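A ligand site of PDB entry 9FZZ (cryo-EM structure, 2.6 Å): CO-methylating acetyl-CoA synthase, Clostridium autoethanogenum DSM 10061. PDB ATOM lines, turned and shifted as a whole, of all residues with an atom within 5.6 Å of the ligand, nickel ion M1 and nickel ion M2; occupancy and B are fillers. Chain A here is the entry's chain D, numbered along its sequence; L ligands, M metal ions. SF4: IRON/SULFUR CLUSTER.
N of Cys 576 is bound to nickel ion M2 (1.9 Å).
Nickel ion M2 is bound by the backbone nitrogen (N) of Gly 575, 2.0 Å away.
The side-chain sulfur (SG) of Cys 574 binds nickel ion M2.
Nickel ion M2 is bound by SG of Cys 576.
Leu 506 touches nickel ion M1.
Four residues have an atom within 4 Å of nickel ion M1: Cys 488, Leu 506, Cys 574 and Cys 576.
O of Cys 497 lies within hydrogen-bond range of N of Cys 485.
SG of Cys 497 lies close to NE2 of His 495.
N of Leu 487 lies close to SG of Cys 485 (3.7 Å).
O of His 495 sits close to NE2 of Gln 489 (3.1 Å).
O of Val 510 lies within hydrogen-bond range of N of Gly 505, 3.0 Å away.
The side-chain sulfur (SG) of Cys 574 lies close to a ring nitrogen (NE2) of His 495, 3.6 Å away.
Phe 491 touches nickel ion M2.
Leu 506 touches nickel ion M2.
Phe 577 touches nickel ion M2 (N to NI, 3.6 Å).
Within 4 Å of nickel ion M2: Phe 491, Leu 506, Cys 574, Gly 575, Cys 576 and Phe 577.
SG of Cys 488 binds nickel ion M1, at 2.1 Å.
SG of Cys 576 binds nickel ion M1 (2.1 Å).
S1 of the ligand is bound to nickel ion M1, 2.2 Å away.
Nickel ion M1 is bound by the side-chain sulfur (SG) of Cys 574 (2.2 Å).
Nickel ion M1 has four donor atoms within binding distance.
SG of Cys 497 binds FE2 of the ligand (2.3 Å).
The backbone NH (N) of Cys 507 lies close to a sulfur (S1) of the ligand, 3.4 Å away.
The side-chain sulfur (SG) of Cys 485 binds an iron atom (FE1) of the ligand (2.3 Å).
N of Cys 488 lies close to S3 of the ligand (3.6 Å).
N of Leu 487 sits close to S3 of the ligand, at 3.5 Å.
SG of Cys 507 binds FE3 of the ligand.
FE4 of the ligand is bound by SG of Cys 488, 2.3 Å away.
His 495 touches the ligand.
Leu 506 touches the ligand.
Val 510 touches the ligand (CB to S4, 3.7 Å).
Hydrophobic or aromatic side chains that line the ligand: Leu 487, Leu 506 and Val 510.
Ten residues have an atom within 4 Å of the ligand: Cys 485, Leu 487, Cys 488, His 495, Cys 497, Leu 506, Cys 507, Val 510, Cys 574 and Cys 576.
The nearest printed residue that does not touch the ligand is Gly 505 (4.02 Å).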
ATOM      1  N   CYS A 485      -7.713  27.394  31.732  1.00  0.00           N
ATOM      2  CA  CYS A 485      -8.536  28.507  31.297  1.00  0.00           C
ATOM      3  C   CYS A 485      -9.963  28.011  31.147  1.00  0.00           C
ATOM      4  O   CYS A 485     -10.200  26.956  30.551  1.00  0.00           O
ATOM      5  CB  CYS A 485      -8.018  29.075  29.971  1.00  0.00           C
ATOM      6  SG  CYS A 485      -8.806  30.620  29.454  1.00  0.00           S
ATOM      7  N   ASN A 486     -10.928  28.760  31.700  1.00  0.00           N
ATOM      8  CA  ASN A 486     -12.348  28.454  31.600  1.00  0.00           C
ATOM      9  C   ASN A 486     -13.124  29.605  30.978  1.00  0.00           C
ATOM     10  O   ASN A 486     -14.301  29.819  31.282  1.00  0.00           O
ATOM     11  CB  ASN A 486     -12.941  28.074  32.957  1.00  0.00           C
ATOM     12  CG  ASN A 486     -12.788  29.171  33.993  1.00  0.00           C
ATOM     13  OD1 ASN A 486     -12.528  30.316  33.658  1.00  0.00           O
ATOM     14  ND2 ASN A 486     -12.961  28.828  35.264  1.00  0.00           N
ATOM     15  N   LEU A 487     -12.477  30.365  30.093  1.00  0.00           N
ATOM     16  CA  LEU A 487     -13.129  31.515  29.482  1.00  0.00           C
ATOM     17  C   LEU A 487     -14.271  31.109  28.562  1.00  0.00           C
ATOM     18  O   LEU A 487     -15.187  31.912  28.347  1.00  0.00           O
ATOM     19  CB  LEU A 487     -12.099  32.352  28.717  1.00  0.00           C
ATOM     20  CG  LEU A 487     -12.569  33.724  28.204  1.00  0.00           C
ATOM     21  CD1 LEU A 487     -13.002  34.615  29.359  1.00  0.00           C
ATOM     22  CD2 LEU A 487     -11.450  34.385  27.423  1.00  0.00           C
ATOM     23  N   CYS A 488     -14.245  29.903  28.020  1.00  0.00           N
ATOM     24  CA  CYS A 488     -15.284  29.414  27.129  1.00  0.00           C
ATOM     25  C   CYS A 488     -16.411  28.724  27.884  1.00  0.00           C
ATOM     26  O   CYS A 488     -17.302  28.145  27.254  1.00  0.00           O
ATOM     27  CB  CYS A 488     -14.702  28.454  26.093  1.00  0.00           C
ATOM     28  SG  CYS A 488     -13.612  29.236  24.897  1.00  0.00           S
ATOM     29  N   GLN A 489     -16.381  28.734  29.214  1.00  0.00           N
ATOM     30  CA  GLN A 489     -17.484  28.178  29.984  1.00  0.00           C
ATOM     31  C   GLN A 489     -18.737  29.028  29.905  1.00  0.00           C
ATOM     32  O   GLN A 489     -19.796  28.592  30.357  1.00  0.00           O
ATOM     33  CB  GLN A 489     -17.075  28.004  31.443  1.00  0.00           C
ATOM     34  CG  GLN A 489     -16.181  26.783  31.661  1.00  0.00           C
ATOM     35  CD  GLN A 489     -16.140  26.372  33.106  1.00  0.00           C
ATOM     36  OE1 GLN A 489     -16.679  27.072  33.959  1.00  0.00           O
ATOM     37  NE2 GLN A 489     -15.520  25.246  33.406  1.00  0.00           N
ATOM     38  N   PHE A 491     -20.329  29.566  27.228  1.00  0.00           N
ATOM     39  CA  PHE A 491     -21.163  28.784  26.321  1.00  0.00           C
ATOM     40  C   PHE A 491     -20.934  27.271  26.386  1.00  0.00           C
ATOM     41  O   PHE A 491     -21.731  26.525  25.816  1.00  0.00           O
ATOM     42  CB  PHE A 491     -20.982  29.256  24.867  1.00  0.00           C
ATOM     43  CG  PHE A 491     -19.586  29.108  24.342  1.00  0.00           C
ATOM     44  CD1 PHE A 491     -18.646  30.123  24.543  1.00  0.00           C
ATOM     45  CD2 PHE A 491     -19.215  27.976  23.637  1.00  0.00           C
ATOM     46  CE1 PHE A 491     -17.346  30.001  24.062  1.00  0.00           C
ATOM     47  CE2 PHE A 491     -17.919  27.840  23.143  1.00  0.00           C
ATOM     48  CZ  PHE A 491     -16.979  28.855  23.358  1.00  0.00           C
ATOM     49  N   HIS A 495     -16.449  22.828  29.881  1.00  0.00           N
ATOM     50  CA  HIS A 495     -15.154  22.867  29.217  1.00  0.00           C
ATOM     51  C   HIS A 495     -14.086  23.515  30.094  1.00  0.00           C
ATOM     52  O   HIS A 495     -14.280  24.630  30.588  1.00  0.00           O
ATOM     53  CB  HIS A 495     -15.249  23.625  27.895  1.00  0.00           C
ATOM     54  CG  HIS A 495     -13.920  23.801  27.211  1.00  0.00           C
ATOM     55  ND1 HIS A 495     -13.153  22.743  26.803  1.00  0.00           N
ATOM     56  CD2 HIS A 495     -13.214  24.909  26.906  1.00  0.00           C
ATOM     57  CE1 HIS A 495     -12.033  23.182  26.256  1.00  0.00           C
ATOM     58  NE2 HIS A 495     -12.048  24.509  26.312  1.00  0.00           N
ATOM     59  N   VAL A 496     -12.955  22.830  30.241  1.00  0.00           N
ATOM     60  CA  VAL A 496     -11.758  23.355  30.886  1.00  0.00           C
ATOM     61  C   VAL A 496     -10.602  23.153  29.923  1.00  0.00           C
ATOM     62  O   VAL A 496     -10.328  22.021  29.498  1.00  0.00           O
ATOM     63  CB  VAL A 496     -11.462  22.657  32.220  1.00  0.00           C
ATOM     64  CG1 VAL A 496     -10.279  23.326  32.909  1.00  0.00           C
ATOM     65  CG2 VAL A 496     -12.682  22.690  33.127  1.00  0.00           C
ATOM     66  N   CYS A 497      -9.915  24.234  29.563  1.00  0.00           N
ATOM     67  CA  CYS A 497      -8.754  24.166  28.695  1.00  0.00           C
ATOM     68  C   CYS A 497      -7.496  24.050  29.539  1.00  0.00           C
ATOM     69  O   CYS A 497      -7.285  24.856  30.450  1.00  0.00           O
ATOM     70  CB  CYS A 497      -8.647  25.404  27.802  1.00  0.00           C
ATOM     71  SG  CYS A 497      -9.132  25.133  26.093  1.00  0.00           S
ATOM     72  N   VAL A 499      -3.624  24.381  29.266  1.00  0.00           N
ATOM     73  CA  VAL A 499      -2.587  24.965  28.426  1.00  0.00           C
ATOM     74  C   VAL A 499      -1.234  24.476  28.956  1.00  0.00           C
ATOM     75  O   VAL A 499      -0.915  24.662  30.135  1.00  0.00           O
ATOM     76  CB  VAL A 499      -2.667  26.489  28.441  1.00  0.00           C
ATOM     77  CG1 VAL A 499      -1.671  27.085  27.467  1.00  0.00           C
ATOM     78  CG2 VAL A 499      -4.073  26.957  28.098  1.00  0.00           C
ATOM     79  N   GLY A 505      -3.909  26.453  23.751  1.00  0.00           N
ATOM     80  CA  GLY A 505      -5.344  26.596  23.952  1.00  0.00           C
ATOM     81  C   GLY A 505      -6.058  26.450  22.621  1.00  0.00           C
ATOM     82  O   GLY A 505      -5.663  27.079  21.636  1.00  0.00           O
ATOM     83  N   LEU A 506      -7.111  25.632  22.571  1.00  0.00           N
ATOM     84  CA  LEU A 506      -7.684  25.264  21.286  1.00  0.00           C
ATOM     85  C   LEU A 506      -8.353  26.435  20.582  1.00  0.00           C
ATOM     86  O   LEU A 506      -8.663  26.327  19.392  1.00  0.00           O
ATOM     87  CB  LEU A 506      -8.666  24.094  21.439  1.00  0.00           C
ATOM     88  CG  LEU A 506      -9.713  24.144  22.545  1.00  0.00           C
ATOM     89  CD1 LEU A 506     -10.929  24.849  22.031  1.00  0.00           C
ATOM     90  CD2 LEU A 506     -10.070  22.729  22.985  1.00  0.00           C
ATOM     91  N   CYS A 507      -8.572  27.558  21.267  1.00  0.00           N
ATOM     92  CA  CYS A 507      -8.984  28.768  20.582  1.00  0.00           C
ATOM     93  C   CYS A 507      -7.860  29.329  19.712  1.00  0.00           C
ATOM     94  O   CYS A 507      -8.139  30.101  18.785  1.00  0.00           O
ATOM     95  CB  CYS A 507      -9.439  29.825  21.582  1.00  0.00           C
ATOM     96  SG  CYS A 507      -8.159  30.309  22.735  1.00  0.00           S
ATOM     97  N   GLY A 508      -6.606  28.962  19.992  1.00  0.00           N
ATOM     98  CA  GLY A 508      -5.476  29.417  19.218  1.00  0.00           C
ATOM     99  C   GLY A 508      -4.880  30.726  19.666  1.00  0.00           C
ATOM    100  O   GLY A 508      -3.825  31.109  19.152  1.00  0.00           O
ATOM    101  N   VAL A 510      -4.428  31.538  23.126  1.00  0.00           N
ATOM    102  CA  VAL A 510      -3.886  31.406  24.474  1.00  0.00           C
ATOM    103  C   VAL A 510      -2.734  30.414  24.420  1.00  0.00           C
ATOM    104  O   VAL A 510      -2.906  29.276  23.952  1.00  0.00           O
ATOM    105  CB  VAL A 510      -4.950  30.946  25.487  1.00  0.00           C
ATOM    106  CG1 VAL A 510      -4.361  30.877  26.887  1.00  0.00           C
ATOM    107  CG2 VAL A 510      -6.136  31.891  25.465  1.00  0.00           C
ATOM    108  N   SER A 573     -13.925  20.014  24.185  1.00  0.00           N
ATOM    109  CA  SER A 573     -13.817  21.134  23.253  1.00  0.00           C
ATOM    110  C   SER A 573     -15.034  22.023  23.419  1.00  0.00           C
ATOM    111  O   SER A 573     -16.125  21.553  23.768  1.00  0.00           O
ATOM    112  CB  SER A 573     -13.760  20.665  21.790  1.00  0.00           C
ATOM    113  OG  SER A 573     -12.630  19.845  21.546  1.00  0.00           O
ATOM    114  N   CYS A 574     -14.846  23.323  23.208  1.00  0.00           N
ATOM    115  CA  CYS A 574     -15.929  24.295  23.367  1.00  0.00           C
ATOM    116  C   CYS A 574     -16.593  24.633  22.043  1.00  0.00           C
ATOM    117  O   CYS A 574     -17.769  24.320  21.836  1.00  0.00           O
ATOM    118  CB  CYS A 574     -15.402  25.552  24.067  1.00  0.00           C
ATOM    119  SG  CYS A 574     -13.763  26.044  23.538  1.00  0.00           S
ATOM    120  N   GLY A 575     -15.841  25.160  21.079  1.00  0.00           N
ATOM    121  CA  GLY A 575     -16.468  25.603  19.843  1.00  0.00           C
ATOM    122  C   GLY A 575     -15.714  26.693  19.112  1.00  0.00           C
ATOM    123  O   GLY A 575     -16.074  27.075  17.997  1.00  0.00           O
ATOM    124  N   CYS A 576     -14.643  27.169  19.727  1.00  0.00           N
ATOM    125  CA  CYS A 576     -13.727  28.115  19.117  1.00  0.00           C
ATOM    126  C   CYS A 576     -12.613  27.442  18.337  1.00  0.00           C
ATOM    127  O   CYS A 576     -11.823  28.134  17.678  1.00  0.00           O
ATOM    128  CB  CYS A 576     -13.109  29.003  20.211  1.00  0.00           C
ATOM    129  SG  CYS A 576     -12.776  28.069  21.709  1.00  0.00           S
ATOM    130  N   PHE A 577     -12.544  26.113  18.358  1.00  0.00           N
ATOM    131  CA  PHE A 577     -11.437  25.399  17.757  1.00  0.00           C
ATOM    132  C   PHE A 577     -11.406  25.606  16.240  1.00  0.00           C
ATOM    133  O   PHE A 577     -12.447  25.625  15.584  1.00  0.00           O
ATOM    134  CB  PHE A 577     -11.514  23.916  18.085  1.00  0.00           C
ATOM    135  CG  PHE A 577     -12.906  23.350  18.029  1.00  0.00           C
ATOM    136  CD1 PHE A 577     -13.489  23.017  16.814  1.00  0.00           C
ATOM    137  CD2 PHE A 577     -13.638  23.171  19.198  1.00  0.00           C
ATOM    138  CE1 PHE A 577     -14.784  22.507  16.760  1.00  0.00           C
ATOM    139  CE2 PHE A 577     -14.943  22.658  19.166  1.00  0.00           C
ATOM    140  CZ  PHE A 577     -15.516  22.328  17.929  1.00  0.00           C
HETATM  141 FE1  SF4 L   1      -9.441  29.824  27.395  1.00  0.00          FE
HETATM  142 FE2  SF4 L   1      -9.541  27.351  26.239  1.00  0.00          FE
HETATM  143 FE3  SF4 L   1      -8.938  29.545  24.728  1.00  0.00          FE
HETATM  144 FE4  SF4 L   1     -11.479  29.204  25.683  1.00  0.00          FE
HETATM  145  S1  SF4 L   1     -10.382  27.868  24.185  1.00  0.00           S
HETATM  146  S2  SF4 L   1     -10.253  31.124  25.706  1.00  0.00           S
HETATM  147  S3  SF4 L   1     -11.052  28.234  27.696  1.00  0.00           S
HETATM  148  S4  SF4 L   1      -7.703  28.695  26.443  1.00  0.00           S
HETATM  149 NI    NI M   1     -12.501  27.884  23.782  1.00  0.00          NI
HETATM  150 NI    NI M   2     -14.379  26.512  21.471  1.00  0.00          NI
